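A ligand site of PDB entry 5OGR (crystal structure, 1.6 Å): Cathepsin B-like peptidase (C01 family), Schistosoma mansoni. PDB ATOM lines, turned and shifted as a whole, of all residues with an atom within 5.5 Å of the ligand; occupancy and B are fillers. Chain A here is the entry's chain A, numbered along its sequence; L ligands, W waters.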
ATOM      1  N   GLN A  25      -3.903  29.086   5.453  1.00  0.00           N
ATOM      2  CA  GLN A  25      -2.532  29.237   4.917  1.00  0.00           C
ATOM      3  C   GLN A  25      -2.361  30.499   4.111  1.00  0.00           C
ATOM      4  O   GLN A  25      -1.221  30.900   3.822  1.00  0.00           O
ATOM      5  CB  GLN A  25      -2.207  28.133   3.908  1.00  0.00           C
ATOM      6  CG  GLN A  25      -1.988  26.738   4.422  1.00  0.00           C
ATOM      7  CD  GLN A  25      -1.961  25.724   3.286  1.00  0.00           C
ATOM      8  OE1 GLN A  25      -1.048  25.726   2.462  1.00  0.00           O
ATOM      9  NE2 GLN A  25      -2.985  24.868   3.228  1.00  0.00           N
ATOM     10  N   CYS A  28       0.063  30.981   0.118  1.00  0.00           N
ATOM     11  CA  CYS A  28       1.407  30.449   0.473  1.00  0.00           C
ATOM     12  C   CYS A  28       1.191  28.943   0.493  1.00  0.00           C
ATOM     13  O   CYS A  28       0.248  28.508   1.151  1.00  0.00           O
ATOM     14  CB  CYS A  28       1.865  31.012   1.861  1.00  0.00           C
ATOM     15  SG  CYS A  28       3.353  30.290   2.558  1.00  0.00           S
ATOM     16  N   GLY A  29       2.084  28.135  -0.088  1.00  0.00           N
ATOM     17  CA  GLY A  29       2.048  26.669   0.013  1.00  0.00           C
ATOM     18  C   GLY A  29       2.621  26.130   1.288  1.00  0.00           C
ATOM     19  O   GLY A  29       3.488  25.217   1.310  1.00  0.00           O
ATOM     20  N   SER A  30       2.106  26.656   2.405  1.00  0.00           N
ATOM     21  CA  SER A  30       2.596  26.326   3.739  1.00  0.00           C
ATOM     22  C   SER A  30       1.814  25.193   4.429  1.00  0.00           C
ATOM     23  O   SER A  30       1.959  24.986   5.647  1.00  0.00           O
ATOM     24  CB  SER A  30       2.595  27.550   4.636  1.00  0.00           C
ATOM     25  OG  SER A  30       1.338  28.234   4.547  1.00  0.00           O
ATOM     26  N   CYS A  31       1.016  24.470   3.653  1.00  0.00           N
ATOM     27  CA  CYS A  31       0.242  23.390   4.198  1.00  0.00           C
ATOM     28  C   CYS A  31       1.041  22.477   5.097  1.00  0.00           C
ATOM     29  O   CYS A  31       0.585  22.020   6.174  1.00  0.00           O
ATOM     30  CB  CYS A  31      -0.444  22.598   3.094  1.00  0.00           C
ATOM     31  SG  CYS A  31       0.707  21.846   1.910  1.00  0.00           S
ATOM     32  N   TRP A  32       2.238  22.099   4.630  1.00  0.00           N
ATOM     33  CA  TRP A  32       3.133  21.235   5.380  1.00  0.00           C
ATOM     34  C   TRP A  32       3.369  21.738   6.816  1.00  0.00           C
ATOM     35  O   TRP A  32       3.380  20.950   7.753  1.00  0.00           O
ATOM     36  CB  TRP A  32       4.471  21.125   4.621  1.00  0.00           C
ATOM     37  CG  TRP A  32       5.258  22.393   4.482  1.00  0.00           C
ATOM     38  CD1 TRP A  32       5.166  23.349   3.511  1.00  0.00           C
ATOM     39  CD2 TRP A  32       6.220  22.884   5.428  1.00  0.00           C
ATOM     40  NE1 TRP A  32       6.047  24.374   3.771  1.00  0.00           N
ATOM     41  CE2 TRP A  32       6.718  24.082   4.941  1.00  0.00           C
ATOM     42  CE3 TRP A  32       6.728  22.362   6.630  1.00  0.00           C
ATOM     43  CZ2 TRP A  32       7.669  24.816   5.647  1.00  0.00           C
ATOM     44  CZ3 TRP A  32       7.651  23.084   7.349  1.00  0.00           C
ATOM     45  CH2 TRP A  32       8.121  24.280   6.846  1.00  0.00           C
ATOM     46  N   CYS A  68      13.386  21.873   5.909  1.00  0.00           N
ATOM     47  CA  CYS A  68      11.956  21.556   5.687  1.00  0.00           C
ATOM     48  C   CYS A  68      11.450  21.799   4.238  1.00  0.00           C
ATOM     49  O   CYS A  68      10.249  21.669   3.983  1.00  0.00           O
ATOM     50  CB  CYS A  68      11.070  22.381   6.667  1.00  0.00           C
ATOM     51  SG  CYS A  68      11.105  21.734   8.350  1.00  0.00           S
ATOM     52  N   GLY A  69      12.344  22.091   3.291  1.00  0.00           N
ATOM     53  CA  GLY A  69      11.909  22.394   1.924  1.00  0.00           C
ATOM     54  C   GLY A  69      12.024  23.838   1.479  1.00  0.00           C
ATOM     55  O   GLY A  69      13.011  24.556   1.799  1.00  0.00           O
ATOM     56  N   LEU A  70      11.018  24.239   0.714  1.00  0.00           N
ATOM     57  CA  LEU A  70      10.967  25.469  -0.027  1.00  0.00           C
ATOM     58  C   LEU A  70       9.983  26.546   0.501  1.00  0.00           C
ATOM     59  O   LEU A  70       9.574  27.507  -0.244  1.00  0.00           O
ATOM     60  CB  LEU A  70      10.592  25.147  -1.466  1.00  0.00           C
ATOM     61  CG  LEU A  70      11.426  24.049  -2.117  1.00  0.00           C
ATOM     62  CD1 LEU A  70      10.911  23.894  -3.558  1.00  0.00           C
ATOM     63  CD2 LEU A  70      12.958  24.359  -2.130  1.00  0.00           C
ATOM     64  N   CYS A  72       7.056  28.691   1.258  1.00  0.00           N
ATOM     65  CA  CYS A  72       5.780  28.852   0.590  1.00  0.00           C
ATOM     66  C   CYS A  72       5.654  28.060  -0.714  1.00  0.00           C
ATOM     67  O   CYS A  72       4.559  27.975  -1.275  1.00  0.00           O
ATOM     68  CB  CYS A  72       5.455  30.331   0.329  1.00  0.00           C
ATOM     69  SG  CYS A  72       4.986  31.299   1.782  1.00  0.00           S
ATOM     70  N   GLU A  73       6.783  27.491  -1.170  1.00  0.00           N
ATOM     71  CA  GLU A  73       6.795  26.673  -2.389  1.00  0.00           C
ATOM     72  C   GLU A  73       6.817  25.180  -2.092  1.00  0.00           C
ATOM     73  O   GLU A  73       7.049  24.355  -2.962  1.00  0.00           O
ATOM     74  CB  GLU A  73       7.982  27.091  -3.272  1.00  0.00           C
ATOM     75  CG  GLU A  73       7.907  28.523  -3.712  1.00  0.00           C
ATOM     76  CD  GLU A  73       6.810  28.842  -4.713  1.00  0.00           C
ATOM     77  OE1 GLU A  73       6.385  27.967  -5.521  1.00  0.00           O
ATOM     78  OE2 GLU A  73       6.388  30.028  -4.747  1.00  0.00           O
ATOM     79  N   GLY A  74       6.502  24.809  -0.858  1.00  0.00           N
ATOM     80  CA  GLY A  74       6.269  23.389  -0.519  1.00  0.00           C
ATOM     81  C   GLY A  74       7.302  22.830   0.454  1.00  0.00           C
ATOM     82  O   GLY A  74       8.488  23.204   0.446  1.00  0.00           O
ATOM     83  N   GLY A  75       6.850  21.909   1.283  1.00  0.00           N
ATOM     84  CA  GLY A  75       7.648  21.391   2.360  1.00  0.00           C
ATOM     85  C   GLY A  75       7.514  19.923   2.691  1.00  0.00           C
ATOM     86  O   GLY A  75       6.743  19.171   2.129  1.00  0.00           O
ATOM     87  N   ILE A  76       8.291  19.524   3.678  1.00  0.00           N
ATOM     88  CA  ILE A  76       8.586  18.118   3.982  1.00  0.00           C
ATOM     89  C   ILE A  76       8.120  17.846   5.415  1.00  0.00           C
ATOM     90  O   ILE A  76       8.511  18.536   6.345  1.00  0.00           O
ATOM     91  CB  ILE A  76      10.068  17.825   3.840  1.00  0.00           C
ATOM     92  CG1 ILE A  76      10.634  18.458   2.576  1.00  0.00           C
ATOM     93  CG2 ILE A  76      10.287  16.309   3.787  1.00  0.00           C
ATOM     94  CD1 ILE A  76      12.155  18.302   2.458  1.00  0.00           C
ATOM     95  N   LEU A  77       7.299  16.817   5.568  1.00  0.00           N
ATOM     96  CA  LEU A  77       6.592  16.578   6.866  1.00  0.00           C
ATOM     97  C   LEU A  77       7.508  16.072   7.996  1.00  0.00           C
ATOM     98  O   LEU A  77       7.494  16.586   9.113  1.00  0.00           O
ATOM     99  CB  LEU A  77       5.446  15.578   6.636  1.00  0.00           C
ATOM    100  CG  LEU A  77       4.137  16.173   6.141  1.00  0.00           C
ATOM    101  CD1 LEU A  77       4.318  16.883   4.836  1.00  0.00           C
ATOM    102  CD2 LEU A  77       3.044  15.077   6.088  1.00  0.00           C
ATOM    103  N   ILE A 124       1.549  33.651  -5.172  1.00  0.00           N
ATOM    104  CA  ILE A 124       2.103  33.016  -3.964  1.00  0.00           C
ATOM    105  C   ILE A 124       3.063  34.050  -3.336  1.00  0.00           C
ATOM    106  O   ILE A 124       3.926  34.604  -4.052  1.00  0.00           O
ATOM    107  CB  ILE A 124       2.852  31.686  -4.332  1.00  0.00           C
ATOM    108  CG1 ILE A 124       1.878  30.624  -4.892  1.00  0.00           C
ATOM    109  CG2 ILE A 124       3.611  31.105  -3.139  1.00  0.00           C
ATOM    110  CD1 ILE A 124       0.902  30.048  -3.890  1.00  0.00           C
ATOM    111  N   GLY A 175      -0.053  13.592   4.415  1.00  0.00           N
ATOM    112  CA  GLY A 175       0.090  14.110   3.033  1.00  0.00           C
ATOM    113  C   GLY A 175      -0.750  13.277   2.039  1.00  0.00           C
ATOM    114  O   GLY A 175      -0.926  12.048   2.190  1.00  0.00           O
ATOM    115  N   PHE A 176      -1.276  13.925   1.005  1.00  0.00           N
ATOM    116  CA  PHE A 176      -2.071  13.222   0.013  1.00  0.00           C
ATOM    117  C   PHE A 176      -1.915  13.959  -1.348  1.00  0.00           C
ATOM    118  O   PHE A 176      -1.507  15.122  -1.417  1.00  0.00           O
ATOM    119  CB  PHE A 176      -3.555  13.039   0.415  1.00  0.00           C
ATOM    120  CG  PHE A 176      -4.383  14.277   0.302  1.00  0.00           C
ATOM    121  CD1 PHE A 176      -4.294  15.267   1.258  1.00  0.00           C
ATOM    122  CD2 PHE A 176      -5.210  14.494  -0.805  1.00  0.00           C
ATOM    123  CE1 PHE A 176      -5.072  16.421   1.152  1.00  0.00           C
ATOM    124  CE2 PHE A 176      -5.997  15.648  -0.900  1.00  0.00           C
ATOM    125  CZ  PHE A 176      -5.907  16.602   0.091  1.00  0.00           C
ATOM    126  N   THR A 177      -2.215  13.225  -2.392  1.00  0.00           N
ATOM    127  CA  THR A 177      -2.097  13.680  -3.743  1.00  0.00           C
ATOM    128  C   THR A 177      -3.289  14.521  -4.119  1.00  0.00           C
ATOM    129  O   THR A 177      -4.430  14.039  -4.000  1.00  0.00           O
ATOM    130  CB  THR A 177      -1.953  12.490  -4.694  1.00  0.00           C
ATOM    131  OG1 THR A 177      -0.785  11.772  -4.303  1.00  0.00           O
ATOM    132  CG2 THR A 177      -1.890  12.926  -6.135  1.00  0.00           C
ATOM    133  N   VAL A 178      -3.034  15.715  -4.632  1.00  0.00           N
ATOM    134  CA  VAL A 178      -4.081  16.613  -5.149  1.00  0.00           C
ATOM    135  C   VAL A 178      -4.250  16.445  -6.631  1.00  0.00           C
ATOM    136  O   VAL A 178      -3.295  16.681  -7.376  1.00  0.00           O
ATOM    137  CB  VAL A 178      -3.811  18.074  -4.799  1.00  0.00           C
ATOM    138  CG1 VAL A 178      -4.838  19.001  -5.418  1.00  0.00           C
ATOM    139  CG2 VAL A 178      -3.689  18.234  -3.284  1.00  0.00           C
ATOM    140  N   LEU A 183     -10.072  20.447  -6.030  1.00  0.00           N
ATOM    141  CA  LEU A 183     -10.229  21.868  -5.910  1.00  0.00           C
ATOM    142  C   LEU A 183     -11.687  22.279  -6.050  1.00  0.00           C
ATOM    143  O   LEU A 183     -12.049  23.398  -5.694  1.00  0.00           O
ATOM    144  CB  LEU A 183      -9.339  22.625  -6.913  1.00  0.00           C
ATOM    145  CG  LEU A 183      -7.848  22.317  -6.820  1.00  0.00           C
ATOM    146  CD1 LEU A 183      -7.126  23.272  -7.777  1.00  0.00           C
ATOM    147  CD2 LEU A 183      -7.264  22.387  -5.433  1.00  0.00           C
ATOM    148  N   LEU A 198      -1.951  17.418  -9.728  1.00  0.00           N
ATOM    149  CA  LEU A 198      -1.467  18.756  -9.516  1.00  0.00           C
ATOM    150  C   LEU A 198      -0.272  18.834  -8.584  1.00  0.00           C
ATOM    151  O   LEU A 198       0.677  19.565  -8.842  1.00  0.00           O
ATOM    152  CB  LEU A 198      -2.576  19.692  -8.996  1.00  0.00           C
ATOM    153  CG  LEU A 198      -3.740  19.926  -9.985  1.00  0.00           C
ATOM    154  CD1 LEU A 198      -4.775  20.908  -9.419  1.00  0.00           C
ATOM    155  CD2 LEU A 198      -3.262  20.457 -11.304  1.00  0.00           C
ATOM    156  N   GLY A 199      -0.302  18.082  -7.484  1.00  0.00           N
ATOM    157  CA  GLY A 199       0.741  18.226  -6.458  1.00  0.00           C
ATOM    158  C   GLY A 199       0.322  17.483  -5.231  1.00  0.00           C
ATOM    159  O   GLY A 199      -0.370  16.502  -5.333  1.00  0.00           O
ATOM    160  N   GLY A 200       0.773  17.967  -4.078  1.00  0.00           N
ATOM    161  CA  GLY A 200       0.424  17.300  -2.810  1.00  0.00           C
ATOM    162  C   GLY A 200      -0.021  18.333  -1.790  1.00  0.00           C
ATOM    163  O   GLY A 200       0.339  19.516  -1.849  1.00  0.00           O
ATOM    164  N   HIS A 201      -0.811  17.850  -0.835  1.00  0.00           N
ATOM    165  CA  HIS A 201      -1.335  18.714   0.212  1.00  0.00           C
ATOM    166  C   HIS A 201      -1.126  17.969   1.542  1.00  0.00           C
ATOM    167  O   HIS A 201      -1.060  16.763   1.578  1.00  0.00           O
ATOM    168  CB  HIS A 201      -2.811  18.990  -0.088  1.00  0.00           C
ATOM    169  CG  HIS A 201      -3.501  19.985   0.818  1.00  0.00           C
ATOM    170  ND1 HIS A 201      -2.809  20.810   1.689  1.00  0.00           N
ATOM    171  CD2 HIS A 201      -4.809  20.256   0.992  1.00  0.00           C
ATOM    172  CE1 HIS A 201      -3.667  21.554   2.369  1.00  0.00           C
ATOM    173  NE2 HIS A 201      -4.890  21.238   1.962  1.00  0.00           N
ATOM    174  N   ALA A 202      -0.981  18.750   2.610  1.00  0.00           N
ATOM    175  CA  ALA A 202      -0.664  18.241   3.951  1.00  0.00           C
ATOM    176  C   ALA A 202      -1.705  18.830   4.882  1.00  0.00           C
ATOM    177  O   ALA A 202      -1.898  20.036   4.920  1.00  0.00           O
ATOM    178  CB  ALA A 202       0.722  18.693   4.384  1.00  0.00           C
ATOM    179  N   SER A 222      -6.797  23.593   5.945  1.00  0.00           N
ATOM    180  CA  SER A 222      -6.219  24.858   6.352  1.00  0.00           C
ATOM    181  C   SER A 222      -6.535  25.957   5.330  1.00  0.00           C
ATOM    182  O   SER A 222      -5.678  26.772   5.035  1.00  0.00           O
ATOM    183  CB  SER A 222      -4.727  24.732   6.586  1.00  0.00           C
ATOM    184  OG  SER A 222      -4.051  24.157   5.471  1.00  0.00           O
ATOM    185  N   TRP A 223      -7.754  25.957   4.839  1.00  0.00           N
ATOM    186  CA  TRP A 223      -8.264  26.915   3.850  1.00  0.00           C
ATOM    187  C   TRP A 223      -9.450  27.703   4.369  1.00  0.00           C
ATOM    188  O   TRP A 223     -10.275  28.196   3.591  1.00  0.00           O
ATOM    189  CB  TRP A 223      -8.657  26.177   2.570  1.00  0.00           C
ATOM    190  CG  TRP A 223      -7.484  25.582   1.805  1.00  0.00           C
ATOM    191  CD1 TRP A 223      -6.148  25.811   2.024  1.00  0.00           C
ATOM    192  CD2 TRP A 223      -7.548  24.715   0.656  1.00  0.00           C
ATOM    193  NE1 TRP A 223      -5.374  25.098   1.104  1.00  0.00           N
ATOM    194  CE2 TRP A 223      -6.226  24.441   0.249  1.00  0.00           C
ATOM    195  CE3 TRP A 223      -8.608  24.130  -0.060  1.00  0.00           C
ATOM    196  CZ2 TRP A 223      -5.934  23.577  -0.804  1.00  0.00           C
ATOM    197  CZ3 TRP A 223      -8.336  23.298  -1.117  1.00  0.00           C
ATOM    198  CH2 TRP A 223      -7.008  23.037  -1.499  1.00  0.00           C
ATOM    199  N   GLU A 247       1.673   8.897   4.127  1.00  0.00           N
ATOM    200  CA  GLU A 247       2.591   9.934   4.568  1.00  0.00           C
ATOM    201  C   GLU A 247       2.102  10.515   5.910  1.00  0.00           C
ATOM    202  O   GLU A 247       2.124  11.712   6.086  1.00  0.00           O
ATOM    203  CB  GLU A 247       2.593  10.982   3.442  1.00  0.00           C
ATOM    204  CG  GLU A 247       3.584  12.089   3.573  1.00  0.00           C
ATOM    205  CD  GLU A 247       4.977  11.721   3.165  1.00  0.00           C
ATOM    206  OE1 GLU A 247       5.137  10.848   2.290  1.00  0.00           O
ATOM    207  OE2 GLU A 247       5.902  12.348   3.738  1.00  0.00           O
HETATM  208  C1  LIG L   1       5.638  19.814  -1.442  1.00  0.00           C
HETATM  209  N1  LIG L   1       7.042  19.792  -1.518  1.00  0.00           N
HETATM  210  C2  LIG L   1       7.613  20.423  -2.717  1.00  0.00           C
HETATM  211  C3  LIG L   1       9.044  20.866  -2.447  1.00  0.00           C
HETATM  212  N2  LIG L   1       9.834  19.744  -1.960  1.00  0.00           N
HETATM  213  C4  LIG L   1      11.258  20.096  -1.698  1.00  0.00           C
HETATM  214  C5  LIG L   1       9.228  19.179  -0.673  1.00  0.00           C
HETATM  215  C6  LIG L   1       7.790  18.736  -0.891  1.00  0.00           C
HETATM  216  O1  LIG L   1       4.918  20.366  -2.261  1.00  0.00           O
HETATM  217  N3  LIG L   1       5.110  19.193  -0.301  1.00  0.00           N
HETATM  218  C7  LIG L   1       3.669  19.372  -0.059  1.00  0.00           C
HETATM  219  C8  LIG L   1       3.314  18.507   1.183  1.00  0.00           C
HETATM  220  C9  LIG L   1       3.372  17.053   0.901  1.00  0.00           C
HETATM  221  C10 LIG L   1       4.511  16.259   1.093  1.00  0.00           C
HETATM  222  C11 LIG L   1       4.515  14.921   0.740  1.00  0.00           C
HETATM  223  C12 LIG L   1       3.367  14.249   0.231  1.00  0.00           C
HETATM  224  C13 LIG L   1       2.214  15.030   0.066  1.00  0.00           C
HETATM  225  C14 LIG L   1       2.220  16.389   0.398  1.00  0.00           C
HETATM  226  C15 LIG L   1       3.395  20.853   0.190  1.00  0.00           C
HETATM  227  O2  LIG L   1       4.086  21.546   0.984  1.00  0.00           O
HETATM  228  N4  LIG L   1       2.297  21.391  -0.460  1.00  0.00           N
HETATM  229  C16 LIG L   1       1.856  22.754  -0.360  1.00  0.00           C
HETATM  230  C17 LIG L   1       1.840  23.398  -1.760  1.00  0.00           C
HETATM  231  C18 LIG L   1       3.274  23.585  -2.298  1.00  0.00           C
HETATM  232  C19 LIG L   1       3.241  24.259  -3.677  1.00  0.00           C
HETATM  233  C20 LIG L   1       3.026  23.431  -4.808  1.00  0.00           C
HETATM  234  C21 LIG L   1       2.976  24.069  -6.073  1.00  0.00           C
HETATM  235  C22 LIG L   1       3.150  25.433  -6.188  1.00  0.00           C
HETATM  236  C23 LIG L   1       3.401  26.271  -5.063  1.00  0.00           C
HETATM  237  C24 LIG L   1       3.413  25.638  -3.816  1.00  0.00           C
HETATM  238  C25 LIG L   1      -0.705  22.417  -0.447  1.00  0.00           C
HETATM  239  S1  LIG L   1      -1.760  23.791  -0.868  1.00  0.00           S
HETATM  240  N5  LIG L   1      -2.191  23.494  -2.461  1.00  0.00           N
HETATM  241  O3  LIG L   1      -2.889  22.286  -2.606  1.00  0.00           O
HETATM  242  C26 LIG L   1      -2.174  21.426  -3.589  1.00  0.00           C
HETATM  243  C27 LIG L   1      -1.725  21.926  -4.941  1.00  0.00           C
HETATM  244  C28 LIG L   1      -0.392  21.679  -5.340  1.00  0.00           C
HETATM  245  C29 LIG L   1       0.070  22.111  -6.586  1.00  0.00           C
HETATM  246  C30 LIG L   1      -0.794  22.782  -7.456  1.00  0.00           C
HETATM  247  C31 LIG L   1      -2.118  23.000  -7.085  1.00  0.00           C
HETATM  248  C32 LIG L   1      -2.583  22.597  -5.846  1.00  0.00           C
HETATM  249  O4  LIG L   1      -2.795  24.077   0.155  1.00  0.00           O
HETATM  250  O5  LIG L   1      -0.955  24.970  -0.981  1.00  0.00           O
HETATM  251  C33 LIG L   1       0.504  22.850   0.425  1.00  0.00           C
HETATM  252  O   HOH W   1      -2.453  27.457   0.378  1.00  0.00           O
HETATM  253  O   HOH W   2      10.291  16.966  -2.827  1.00  0.00           O
HETATM  254  O   HOH W   3      -4.531  25.446  -3.391  1.00  0.00           O
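O of Val 178 is in hydrogen-bond range of N of Leu 198.
N of His 201 is in hydrogen-bond range of O of Phe 176, 2.9 Å away.
The side-chain sulfur of Cys 31 lies close to a ring nitrogen (ND1) of His 201 (3.7 Å).
The side-chain amide nitrogen of Gln 25 sits at hydrogen-bond distance from the side-chain hydroxyl of Ser 222 (2.6 Å).
The backbone NH of Val 178 lies within hydrogen-bond range of the backbone carbonyl oxygen of Gly 199.
The backbone NH of Ser 30 sits at hydrogen-bond distance from the side-chain amide oxygen of Gln 25 (3.3 Å).
The backbone carbonyl oxygen of Cys 68 lies within hydrogen-bond range of the backbone NH of Ile 76, at 2.9 Å.
SG of Cys 31 is in hydrogen-bond range of N of Ala 202 (3.6 Å).
The side-chain amide nitrogen of Gln 25 is in hydrogen-bond range of an oxygen (O4) of the ligand, at 3.2 Å.
An oxygen (O4) of the ligand sits at hydrogen-bond distance from the indole nitrogen of Trp 223 (2.9 Å).
A nitrogen (N4) of the ligand lies within hydrogen-bond range of the backbone carbonyl oxygen (O) of Gly 200 (3.0 Å).
The side-chain sulfur (SG) of Cys 31 is covalently linked to a carbon (C33) of the ligand (1.8 Å).
The backbone NH of Gly 75 sits at hydrogen-bond distance from an oxygen (O2) of the ligand (2.8 Å).
A nitrogen (N3) of the ligand sits at hydrogen-bond distance from the backbone carbonyl oxygen of Gly 75 (2.9 Å).
O of Gly 29 touches C16 of the ligand, at 3.4 Å.
Trp 32 touches the ligand.
Leu 70 touches the ligand (CD1 to C3, 3.7 Å).
Cys 72 touches the ligand (O to C24, 3.6 Å).
OE1 of Glu 73 touches C23 of the ligand, 3.5 Å away.
CA of Gly 74 touches O2 of the ligand, 3.2 Å away.
CG1 of Ile 76 touches C5 of the ligand, 3.6 Å away.
Leu 77 touches the ligand.
Gly 175 touches the ligand (CA to C13, 3.8 Å).
Phe 176 touches the ligand.
CG2 of Val 178 touches C26 of the ligand, 3.5 Å away.
Leu 198 touches the ligand (O to C29, 3.5 Å).
CA of Gly 199 touches C28 of the ligand, at 3.8 Å.
His 201 touches the ligand.
Glu 247 touches the ligand (CG to C12, 3.99 Å).
Hydrophobic or aromatic side chains that line the ligand: Trp 32, Leu 70, Ile 76, Leu 77, Val 178, Leu 198, His 201 and Trp 223.
Of the 29 residues printed, 20 come within 4 Å of the ligand.
The nearest printed residue that does not touch the ligand is Ala 202 (4.1 Å).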
